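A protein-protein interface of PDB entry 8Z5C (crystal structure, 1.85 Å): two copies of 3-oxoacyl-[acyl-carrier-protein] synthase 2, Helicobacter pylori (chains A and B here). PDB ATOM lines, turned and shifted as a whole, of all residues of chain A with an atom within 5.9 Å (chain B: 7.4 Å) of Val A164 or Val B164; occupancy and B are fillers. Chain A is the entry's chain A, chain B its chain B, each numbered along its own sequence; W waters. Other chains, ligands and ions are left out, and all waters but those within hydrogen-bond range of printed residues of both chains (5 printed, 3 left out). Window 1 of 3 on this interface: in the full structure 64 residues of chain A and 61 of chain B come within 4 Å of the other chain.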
ATOM      1  N   SER A 108       1.015  30.693  20.484  1.00  0.00           N
ATOM      2  CA  SER A 108       0.010  30.956  19.465  1.00  0.00           C
ATOM      3  C   SER A 108      -0.008  29.815  18.463  1.00  0.00           C
ATOM      4  O   SER A 108       1.011  29.177  18.214  1.00  0.00           O
ATOM      5  CB  SER A 108       0.266  32.285  18.746  1.00  0.00           C
ATOM      6  OG  SER A 108       1.580  32.362  18.215  1.00  0.00           O
ATOM      7  N   GLY A 109      -1.169  29.532  17.910  1.00  0.00           N
ATOM      8  CA  GLY A 109      -1.289  28.476  16.920  1.00  0.00           C
ATOM      9  C   GLY A 109      -2.080  28.934  15.714  1.00  0.00           C
ATOM     10  O   GLY A 109      -3.060  29.671  15.841  1.00  0.00           O
ATOM     11  N   SER A 110      -1.650  28.474  14.545  1.00  0.00           N
ATOM     12  CA  SER A 110      -2.406  28.659  13.315  1.00  0.00           C
ATOM     13  C   SER A 110      -1.884  27.635  12.309  1.00  0.00           C
ATOM     14  O   SER A 110      -0.706  27.266  12.346  1.00  0.00           O
ATOM     15  CB  SER A 110      -2.262  30.089  12.785  1.00  0.00           C
ATOM     16  OG  SER A 110      -2.959  30.240  11.562  1.00  0.00           O
ATOM     17  N   GLY A 111      -2.768  27.158  11.437  1.00  0.00           N
ATOM     18  CA  GLY A 111      -2.351  26.191  10.435  1.00  0.00           C
ATOM     19  C   GLY A 111      -1.673  26.865   9.253  1.00  0.00           C
ATOM     20  O   GLY A 111      -0.665  26.372   8.740  1.00  0.00           O
ATOM     21  N   ILE A 112      -2.207  27.999   8.806  1.00  0.00           N
ATOM     22  CA  ILE A 112      -1.711  28.612   7.576  1.00  0.00           C
ATOM     23  C   ILE A 112      -1.417  30.098   7.724  1.00  0.00           C
ATOM     24  O   ILE A 112      -0.736  30.684   6.858  1.00  0.00           O
ATOM     25  CB  ILE A 112      -2.700  28.386   6.412  1.00  0.00           C
ATOM     26  CG1 ILE A 112      -3.196  26.944   6.376  1.00  0.00           C
ATOM     27  CG2 ILE A 112      -1.961  28.555   5.110  1.00  0.00           C
ATOM     28  CD1 ILE A 112      -4.308  26.697   5.336  1.00  0.00           C
ATOM     29  N   LEU A 142       3.035  35.980   8.518  1.00  0.00           N
ATOM     30  CA  LEU A 142       3.742  34.932   9.261  1.00  0.00           C
ATOM     31  C   LEU A 142       2.926  34.486  10.475  1.00  0.00           C
ATOM     32  O   LEU A 142       2.367  35.312  11.194  1.00  0.00           O
ATOM     33  CB  LEU A 142       5.101  35.471   9.720  1.00  0.00           C
ATOM     34  CG  LEU A 142       6.085  35.864   8.613  1.00  0.00           C
ATOM     35  CD1 LEU A 142       7.464  35.941   9.159  1.00  0.00           C
ATOM     36  CD2 LEU A 142       6.056  34.819   7.522  1.00  0.00           C
ATOM     37  N   VAL A 143       2.894  33.172  10.730  1.00  0.00           N
ATOM     38  CA  VAL A 143       2.014  32.641  11.776  1.00  0.00           C
ATOM     39  C   VAL A 143       2.380  33.213  13.143  1.00  0.00           C
ATOM     40  O   VAL A 143       1.501  33.535  13.960  1.00  0.00           O
ATOM     41  CB  VAL A 143       2.078  31.102  11.786  1.00  0.00           C
ATOM     42  CG1 VAL A 143       1.504  30.527  13.080  1.00  0.00           C
ATOM     43  CG2 VAL A 143       1.360  30.532  10.565  1.00  0.00           C
ATOM     44  N   ASN A 144       3.678  33.294  13.439  1.00  0.00           N
ATOM     45  CA  ASN A 144       4.102  33.748  14.765  1.00  0.00           C
ATOM     46  C   ASN A 144       3.841  35.225  14.990  1.00  0.00           C
ATOM     47  O   ASN A 144       4.034  35.705  16.118  1.00  0.00           O
ATOM     48  CB  ASN A 144       5.588  33.445  14.957  1.00  0.00           C
ATOM     49  CG  ASN A 144       6.458  34.347  14.128  1.00  0.00           C
ATOM     50  OD1 ASN A 144       6.422  34.284  12.890  1.00  0.00           O
ATOM     51  ND2 ASN A 144       7.292  35.153  14.786  1.00  0.00           N
ATOM     52  N   SER A 162       5.184  29.441  18.935  1.00  0.00           N
ATOM     53  CA  SER A 162       4.047  29.233  18.025  1.00  0.00           C
ATOM     54  C   SER A 162       3.976  27.721  17.511  1.00  0.00           C
ATOM     55  O   SER A 162       4.965  26.915  17.401  1.00  0.00           O
ATOM     56  CB  SER A 162       4.247  30.270  16.904  1.00  0.00           C
ATOM     57  OG  SER A 162       3.112  30.367  16.075  1.00  0.00           O
ATOM     58  N   SER A 163       2.740  27.327  17.297  1.00  0.00           N
ATOM     59  CA  SER A 163       2.481  25.971  16.836  1.00  0.00           C
ATOM     60  C   SER A 163       1.793  26.043  15.481  1.00  0.00           C
ATOM     61  O   SER A 163       0.942  26.909  15.262  1.00  0.00           O
ATOM     62  CB  SER A 163       1.594  25.205  17.834  1.00  0.00           C
ATOM     63  OG  SER A 163       2.230  25.102  19.102  1.00  0.00           O
ATOM     64  N   VAL A 164       2.148  25.123  14.581  1.00  0.00           N
ATOM     65  CA  VAL A 164       1.650  25.192  13.208  1.00  0.00           C
ATOM     66  C   VAL A 164       1.348  23.771  12.723  1.00  0.00           C
ATOM     67  O   VAL A 164       1.513  23.450  11.545  1.00  0.00           O
ATOM     68  CB  VAL A 164       2.666  25.935  12.304  1.00  0.00           C
ATOM     69  CG1 VAL A 164       4.011  25.177  12.196  1.00  0.00           C
ATOM     70  CG2 VAL A 164       2.081  26.268  10.925  1.00  0.00           C
ATOM     71  N   THR A 165       0.898  22.909  13.636  1.00  0.00           N
ATOM     72  CA  THR A 165       0.484  21.557  13.269  1.00  0.00           C
ATOM     73  C   THR A 165      -0.942  21.469  12.722  1.00  0.00           C
ATOM     74  O   THR A 165      -1.760  20.681  13.213  1.00  0.00           O
ATOM     75  CB  THR A 165       0.673  20.647  14.474  1.00  0.00           C
ATOM     76  OG1 THR A 165       0.295  21.359  15.661  1.00  0.00           O
ATOM     77  CG2 THR A 165       2.132  20.191  14.559  1.00  0.00           C
ATOM     78  N   ALA A 166      -1.237  22.256  11.682  1.00  0.00           N
ATOM     79  CA  ALA A 166      -2.490  22.150  10.894  1.00  0.00           C
ATOM     80  C   ALA A 166      -3.687  22.122  11.844  1.00  0.00           C
ATOM     81  O   ALA A 166      -3.752  22.971  12.743  1.00  0.00           O
ATOM     82  CB  ALA A 166      -2.383  20.955   9.947  1.00  0.00           C
ATOM     83  N   ALA A 169      -3.132  22.653  15.630  1.00  0.00           N
ATOM     84  CA  ALA A 169      -2.254  23.720  16.117  1.00  0.00           C
ATOM     85  C   ALA A 169      -2.797  24.363  17.390  1.00  0.00           C
ATOM     86  O   ALA A 169      -2.025  24.743  18.283  1.00  0.00           O
ATOM     87  CB  ALA A 169      -2.068  24.769  15.018  1.00  0.00           C
ATOM     88  N   SER B 108       9.704  19.884  14.114  1.00  0.00           N
ATOM     89  CA  SER B 108      10.153  20.584  12.884  1.00  0.00           C
ATOM     90  C   SER B 108       9.893  22.120  12.983  1.00  0.00           C
ATOM     91  O   SER B 108       8.972  22.689  13.648  1.00  0.00           O
ATOM     92  CB  SER B 108       9.426  19.973  11.671  1.00  0.00           C
ATOM     93  OG  SER B 108       8.018  19.990  11.808  1.00  0.00           O
ATOM     94  N   GLY B 109      10.817  22.846  12.375  1.00  0.00           N
ATOM     95  CA  GLY B 109      10.684  24.292  12.354  1.00  0.00           C
ATOM     96  C   GLY B 109      10.870  24.833  10.956  1.00  0.00           C
ATOM     97  O   GLY B 109      11.690  24.342  10.192  1.00  0.00           O
ATOM     98  N   SER B 110      10.080  25.848  10.630  1.00  0.00           N
ATOM     99  CA  SER B 110      10.225  26.592   9.388  1.00  0.00           C
ATOM    100  C   SER B 110       9.533  27.924   9.645  1.00  0.00           C
ATOM    101  O   SER B 110       8.590  27.987  10.433  1.00  0.00           O
ATOM    102  CB  SER B 110       9.581  25.844   8.208  1.00  0.00           C
ATOM    103  OG  SER B 110       9.663  26.599   7.004  1.00  0.00           O
ATOM    104  N   GLY B 111      10.012  28.983   8.998  1.00  0.00           N
ATOM    105  CA  GLY B 111       9.356  30.268   9.160  1.00  0.00           C
ATOM    106  C   GLY B 111       8.153  30.434   8.257  1.00  0.00           C
ATOM    107  O   GLY B 111       7.133  30.999   8.676  1.00  0.00           O
ATOM    108  N   ILE B 112       8.252  29.952   7.011  1.00  0.00           N
ATOM    109  CA  ILE B 112       7.214  30.228   6.024  1.00  0.00           C
ATOM    110  C   ILE B 112       6.774  28.996   5.241  1.00  0.00           C
ATOM    111  O   ILE B 112       5.753  29.041   4.550  1.00  0.00           O
ATOM    112  CB  ILE B 112       7.642  31.325   5.030  1.00  0.00           C
ATOM    113  CG1 ILE B 112       8.584  32.334   5.686  1.00  0.00           C
ATOM    114  CG2 ILE B 112       6.389  32.032   4.506  1.00  0.00           C
ATOM    115  CD1 ILE B 112       8.960  33.525   4.794  1.00  0.00           C
ATOM    116  N   GLY B 113       7.518  27.892   5.338  1.00  0.00           N
ATOM    117  CA  GLY B 113       7.013  26.725   4.638  1.00  0.00           C
ATOM    118  C   GLY B 113       7.066  26.899   3.129  1.00  0.00           C
ATOM    119  O   GLY B 113       7.959  27.547   2.589  1.00  0.00           O
ATOM    120  N   LEU B 142       2.224  23.462   3.917  1.00  0.00           N
ATOM    121  CA  LEU B 142       2.054  23.607   5.359  1.00  0.00           C
ATOM    122  C   LEU B 142       3.329  23.214   6.089  1.00  0.00           C
ATOM    123  O   LEU B 142       3.934  22.176   5.792  1.00  0.00           O
ATOM    124  CB  LEU B 142       0.898  22.734   5.848  1.00  0.00           C
ATOM    125  CG  LEU B 142      -0.467  22.984   5.208  1.00  0.00           C
ATOM    126  CD1 LEU B 142      -1.518  22.040   5.829  1.00  0.00           C
ATOM    127  CD2 LEU B 142      -0.851  24.447   5.410  1.00  0.00           C
ATOM    128  N   VAL B 143       3.720  24.032   7.073  1.00  0.00           N
ATOM    129  CA  VAL B 143       5.028  23.863   7.710  1.00  0.00           C
ATOM    130  C   VAL B 143       5.122  22.503   8.399  1.00  0.00           C
ATOM    131  O   VAL B 143       6.164  21.832   8.351  1.00  0.00           O
ATOM    132  CB  VAL B 143       5.294  25.014   8.701  1.00  0.00           C
ATOM    133  CG1 VAL B 143       6.473  24.683   9.621  1.00  0.00           C
ATOM    134  CG2 VAL B 143       5.522  26.338   7.965  1.00  0.00           C
ATOM    135  N   ASN B 144       4.038  22.067   9.040  1.00  0.00           N
ATOM    136  CA  ASN B 144       4.074  20.801   9.771  1.00  0.00           C
ATOM    137  C   ASN B 144       4.151  19.578   8.854  1.00  0.00           C
ATOM    138  O   ASN B 144       4.375  18.459   9.341  1.00  0.00           O
ATOM    139  CB  ASN B 144       2.856  20.735  10.677  1.00  0.00           C
ATOM    140  CG  ASN B 144       1.577  20.414   9.897  1.00  0.00           C
ATOM    141  OD1 ASN B 144       1.110  21.218   9.083  1.00  0.00           O
ATOM    142  ND2 ASN B 144       0.999  19.248  10.167  1.00  0.00           N
ATOM    143  N   MET B 145       4.001  19.748   7.541  1.00  0.00           N
ATOM    144  CA  MET B 145       4.249  18.609   6.657  1.00  0.00           C
ATOM    145  C   MET B 145       5.714  18.196   6.609  1.00  0.00           C
ATOM    146  O   MET B 145       6.004  17.103   6.111  1.00  0.00           O
ATOM    147  CB  MET B 145       3.703  18.900   5.259  1.00  0.00           C
ATOM    148  CG  MET B 145       2.211  19.202   5.288  1.00  0.00           C
ATOM    149  SD  MET B 145       1.317  17.697   5.805  1.00  0.00           S
ATOM    150  CE  MET B 145       2.051  16.567   4.642  1.00  0.00           C
ATOM    151  N   LEU B 161       5.561  17.708  16.439  1.00  0.00           N
ATOM    152  CA  LEU B 161       5.402  19.102  16.830  1.00  0.00           C
ATOM    153  C   LEU B 161       6.081  20.002  15.816  1.00  0.00           C
ATOM    154  O   LEU B 161       7.047  19.611  15.155  1.00  0.00           O
ATOM    155  CB  LEU B 161       6.012  19.340  18.216  1.00  0.00           C
ATOM    156  CG  LEU B 161       5.525  18.295  19.226  1.00  0.00           C
ATOM    157  CD1 LEU B 161       6.227  18.482  20.565  1.00  0.00           C
ATOM    158  CD2 LEU B 161       4.018  18.416  19.366  1.00  0.00           C
ATOM    159  N   SER B 162       5.603  21.241  15.732  1.00  0.00           N
ATOM    160  CA  SER B 162       6.166  22.147  14.749  1.00  0.00           C
ATOM    161  C   SER B 162       6.319  23.533  15.363  1.00  0.00           C
ATOM    162  O   SER B 162       5.535  23.933  16.226  1.00  0.00           O
ATOM    163  CB  SER B 162       5.262  22.157  13.521  1.00  0.00           C
ATOM    164  OG  SER B 162       6.003  22.415  12.355  1.00  0.00           O
ATOM    165  N   SER B 163       7.345  24.261  14.916  1.00  0.00           N
ATOM    166  CA  SER B 163       7.680  25.586  15.424  1.00  0.00           C
ATOM    167  C   SER B 163       7.728  26.549  14.250  1.00  0.00           C
ATOM    168  O   SER B 163       8.229  26.197  13.186  1.00  0.00           O
ATOM    169  CB  SER B 163       9.046  25.570  16.130  1.00  0.00           C
ATOM    170  OG  SER B 163       9.011  24.834  17.339  1.00  0.00           O
ATOM    171  N   VAL B 164       7.209  27.767  14.429  1.00  0.00           N
ATOM    172  CA  VAL B 164       7.060  28.669  13.290  1.00  0.00           C
ATOM    173  C   VAL B 164       7.362  30.099  13.736  1.00  0.00           C
ATOM    174  O   VAL B 164       6.812  31.068  13.208  1.00  0.00           O
ATOM    175  CB  VAL B 164       5.657  28.495  12.665  1.00  0.00           C
ATOM    176  CG1 VAL B 164       4.557  29.000  13.622  1.00  0.00           C
ATOM    177  CG2 VAL B 164       5.549  29.138  11.249  1.00  0.00           C
ATOM    178  N   THR B 165       8.275  30.235  14.693  1.00  0.00           N
ATOM    179  CA  THR B 165       8.719  31.528  15.191  1.00  0.00           C
ATOM    180  C   THR B 165       9.782  32.158  14.292  1.00  0.00           C
ATOM    181  O   THR B 165      10.847  32.556  14.779  1.00  0.00           O
ATOM    182  CB  THR B 165       9.235  31.378  16.626  1.00  0.00           C
ATOM    183  OG1 THR B 165       9.904  30.112  16.761  1.00  0.00           O
ATOM    184  CG2 THR B 165       8.070  31.452  17.644  1.00  0.00           C
ATOM    185  N   ALA B 166       9.496  32.256  12.990  1.00  0.00           N
ATOM    186  CA  ALA B 166      10.309  33.025  12.020  1.00  0.00           C
ATOM    187  C   ALA B 166      11.773  32.612  12.152  1.00  0.00           C
ATOM    188  O   ALA B 166      12.053  31.405  12.132  1.00  0.00           O
ATOM    189  CB  ALA B 166      10.041  34.513  12.214  1.00  0.00           C
ATOM    190  N   CYS B 167      12.708  33.566  12.315  1.00  0.00           N
ATOM    191  CA  CYS B 167      14.155  33.361  12.377  1.00  0.00           C
ATOM    192  C   CYS B 167      14.601  32.509  13.535  1.00  0.00           C
ATOM    193  O   CYS B 167      15.785  32.155  13.588  1.00  0.00           O
ATOM    194  CB  CYS B 167      14.915  34.668  12.625  1.00  0.00           C
ATOM    195  SG  CYS B 167      14.532  36.035  11.637  1.00  0.00           S
ATOM    196  N   ALA B 168      13.737  32.290  14.516  1.00  0.00           N
ATOM    197  CA  ALA B 168      14.086  31.480  15.673  1.00  0.00           C
ATOM    198  C   ALA B 168      13.485  30.080  15.604  1.00  0.00           C
ATOM    199  O   ALA B 168      13.699  29.291  16.530  1.00  0.00           O
ATOM    200  CB  ALA B 168      13.634  32.190  16.952  1.00  0.00           C
ATOM    201  N   ALA B 169      12.753  29.751  14.523  1.00  0.00           N
ATOM    202  CA  ALA B 169      11.998  28.492  14.482  1.00  0.00           C
ATOM    203  C   ALA B 169      12.908  27.280  14.672  1.00  0.00           C
ATOM    204  O   ALA B 169      12.543  26.313  15.351  1.00  0.00           O
ATOM    205  CB  ALA B 169      11.227  28.382  13.161  1.00  0.00           C
ATOM    206  N   GLY B 170      14.086  27.295  14.055  1.00  0.00           N
ATOM    207  CA  GLY B 170      14.965  26.154  14.165  1.00  0.00           C
ATOM    208  C   GLY B 170      15.478  25.935  15.573  1.00  0.00           C
ATOM    209  O   GLY B 170      15.731  24.796  15.970  1.00  0.00           O
ATOM    210  N   HIS B 172      13.772  27.032  18.373  1.00  0.00           N
ATOM    211  CA  HIS B 172      12.625  26.616  19.165  1.00  0.00           C
ATOM    212  C   HIS B 172      12.271  25.163  18.883  1.00  0.00           C
ATOM    213  O   HIS B 172      11.769  24.471  19.777  1.00  0.00           O
ATOM    214  CB  HIS B 172      11.422  27.529  18.896  1.00  0.00           C
ATOM    215  CG  HIS B 172      11.536  28.862  19.564  1.00  0.00           C
ATOM    216  ND1 HIS B 172      11.417  30.054  18.882  1.00  0.00           N
ATOM    217  CD2 HIS B 172      11.845  29.190  20.845  1.00  0.00           C
ATOM    218  CE1 HIS B 172      11.574  31.059  19.729  1.00  0.00           C
ATOM    219  NE2 HIS B 172      11.852  30.563  20.922  1.00  0.00           N
ATOM    220  N   ALA B 173      12.535  24.679  17.660  1.00  0.00           N
ATOM    221  CA  ALA B 173      12.281  23.270  17.375  1.00  0.00           C
ATOM    222  C   ALA B 173      13.148  22.376  18.250  1.00  0.00           C
ATOM    223  O   ALA B 173      12.677  21.347  18.752  1.00  0.00           O
ATOM    224  CB  ALA B 173      12.514  22.976  15.893  1.00  0.00           C
ATOM    225  N   GLU B 176      11.585  22.744  21.994  1.00  0.00           N
ATOM    226  CA  GLU B 176      10.331  22.036  22.242  1.00  0.00           C
ATOM    227  C   GLU B 176      10.564  20.528  22.295  1.00  0.00           C
ATOM    228  O   GLU B 176       9.934  19.821  23.097  1.00  0.00           O
ATOM    229  CB  GLU B 176       9.298  22.394  21.164  1.00  0.00           C
ATOM    230  CG  GLU B 176       7.902  21.834  21.459  1.00  0.00           C
ATOM    231  CD  GLU B 176       6.804  22.353  20.539  1.00  0.00           C
ATOM    232  OE1 GLU B 176       7.106  22.847  19.433  1.00  0.00           O
ATOM    233  OE2 GLU B 176       5.622  22.253  20.923  1.00  0.00           O
ATOM    234  N   GLY B 344      13.852  30.157   9.158  1.00  0.00           N
ATOM    235  CA  GLY B 344      13.468  29.147  10.134  1.00  0.00           C
ATOM    236  C   GLY B 344      14.441  27.993  10.226  1.00  0.00           C
ATOM    237  O   GLY B 344      14.439  27.261  11.224  1.00  0.00           O
ATOM    238  N   PHE B 400      11.838  37.701  13.797  1.00  0.00           N
ATOM    239  CA  PHE B 400      10.793  38.691  13.557  1.00  0.00           C
ATOM    240  C   PHE B 400       9.627  38.473  14.505  1.00  0.00           C
ATOM    241  O   PHE B 400       9.291  37.336  14.842  1.00  0.00           O
ATOM    242  CB  PHE B 400      10.309  38.604  12.111  1.00  0.00           C
ATOM    243  CG  PHE B 400      11.275  39.175  11.131  1.00  0.00           C
ATOM    244  CD1 PHE B 400      12.419  38.466  10.777  1.00  0.00           C
ATOM    245  CD2 PHE B 400      11.052  40.421  10.564  1.00  0.00           C
ATOM    246  CE1 PHE B 400      13.330  38.984   9.875  1.00  0.00           C
ATOM    247  CE2 PHE B 400      11.953  40.954   9.652  1.00  0.00           C
ATOM    248  CZ  PHE B 400      13.100  40.237   9.311  1.00  0.00           C
ATOM    249  N   THR B 403      10.672  37.397  18.850  1.00  0.00           N
ATOM    250  CA  THR B 403      10.725  36.102  19.517  1.00  0.00           C
ATOM    251  C   THR B 403      12.157  35.583  19.550  1.00  0.00           C
ATOM    252  O   THR B 403      12.830  35.521  18.515  1.00  0.00           O
ATOM    253  CB  THR B 403       9.790  35.080  18.864  1.00  0.00           C
ATOM    254  OG1 THR B 403       9.900  33.849  19.588  1.00  0.00           O
ATOM    255  CG2 THR B 403      10.101  34.858  17.383  1.00  0.00           C
HETATM  256  O   HOH W   1       3.658  22.796  19.430  1.00  0.00           O
HETATM  257  O   HOH W   2       3.092  22.060  16.856  1.00  0.00           O
HETATM  258  O   HOH W   3       1.988  26.441   7.404  1.00  0.00           O
HETATM  259  O   HOH W   4       7.692  28.327  18.098  1.00  0.00           O
HETATM  260  O   HOH W   5       4.289  31.461   8.790  1.00  0.00           O
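Water W1 lies within hydrogen-bond range of the side-chain carboxylate (OE2) of Glu B176 (2.5 Å) and the side-chain hydroxyl (OG) of Ser A163 (2.7 Å). Water W4 lies within hydrogen-bond range of the backbone NH of Ser A162 and the side-chain hydroxyl of Thr B165. Water W2 bridges the backbone NH of Ser B162 and the side-chain hydroxyl of Thr A165. Water W5 bridges the backbone carbonyl oxygen of Gly B111 (2.9 Å) and the backbone NH of Val A143 (2.9 Å). Water W3 lies within hydrogen-bond range of the backbone carbonyl oxygen (O) of Gly A111 (3.0 Å) and the backbone NH (N) of Val B143 (3.0 Å).
O of Ser A108 lies close to OG of Ser A162, at 3.2 Å. The backbone NH of Ser A110 is in hydrogen-bond range of the backbone carbonyl oxygen of Ser A163, 3.1 Å away. The backbone carbonyl oxygen of Ser B108 sits at hydrogen-bond distance from the backbone NH of Ser B163. The backbone carbonyl oxygen (O) of Ser B163 is in hydrogen-bond range of the backbone NH (N) of Ser B110 (3.2 Å). OE1 of Glu B176 lies within hydrogen-bond range of OG of Ser B163 (3.5 Å). ND1 of His B172 lies within hydrogen-bond range of OG1 of Thr B165.
Of the 26 printed residues of chain B, 11 touch a printed residue of chain A. Hydrophobic or aromatic side chains of chain B that line the printed part of chain A: Ile B112, Leu B142, Val B143, Val B164 and Ala B166. Printed residues of chain A that touch a printed residue of chain B: Gly A111, Ile A112, Leu A142, Val A143, Asn A144, Ser A162, Ser A163, Val A164, Thr A165 and Ala A166. Along chain A the printed residues that touch a printed residue of chain B span positions 111 to 166. Among the printed residues, 21 pairs touch across the chains.
Asn A144 touches Val B164, and with the chains exchanged Val A164 touches Asn B144. Asn A144 touches Ala B166, and with the chains exchanged Ala A166 touches Asn B144. Ser B162 touches its own counterpart, Ser A162. Ser A162 touches Ser B163, and with the chains exchanged Ser A163 touches Ser B162. Of the 21 pairs that touch across the chains among the printed residues, 18 have their exchanged pair printed and touching as well.
The backbone carbonyl oxygen of Val B164 sits close to the side-chain amide oxygen of Asn A144, at 3.3 Å. The side-chain amide nitrogen (ND2) of Asn A144 is in hydrogen-bond range of the backbone carbonyl oxygen (O) of Phe B400. The backbone carbonyl oxygen (O) of Val A164 sits close to the side-chain amide oxygen (OD1) of Asn B144. O of Ser B162 lies close to O of Ser A162 (3.3 Å).
Of the printed residues of chain B, Gly A111 touches Leu B142. Of the printed residues of chain B, Val A143 touches Val B164 (3.5 Å). Ser B108 touches none of the printed residues of chain A. Printed residues of chain A within 4 Å of Asn B144: Val A164, Thr A165 and Ala A166. Met B145 touches none of the printed residues of chain A. Of the printed residues of chain A, Ser B163 touches Ser A162 (3.6 Å). Of the printed residues of chain A, Val B164 touches Val A143, Asn A144, Ser A162 and Val A164. Of the printed residues of chain A, Thr B165 touches Asn A144 (3.7 Å) and Ser A162 (3.7 Å). The nearest residue of chain B that does not touch Val A164 is Ser B163 (4.4 Å). The nearest printed residue of chain A that does not touch Val B164 is Ser A163 (4.4 Å). The nearest printed residue of chain A that does not touch Leu B142 is Ala A166 (4.3 Å).
O of Gly A111 touches CD2 of Leu B142, at 3.9 Å. Ile A112 touches Leu B142 (CG1 to CD2, 3.6 Å). Val A143 touches Val B164. Asn A144 touches Ala B166. Ser B163 touches Ser A162. Ser A162 touches Thr B165 (N to CG2, 3.7 Å). CA of Ser A163 touches O of Ser B162, 3.7 Å away. Val A164 touches Val B143 (CG1 to CG1, 3.6 Å). N of Ser B162 touches CG2 of Thr A165 (3.8 Å). CB of Ala A166 touches OD1 of Asn B144, at 3.6 Å.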
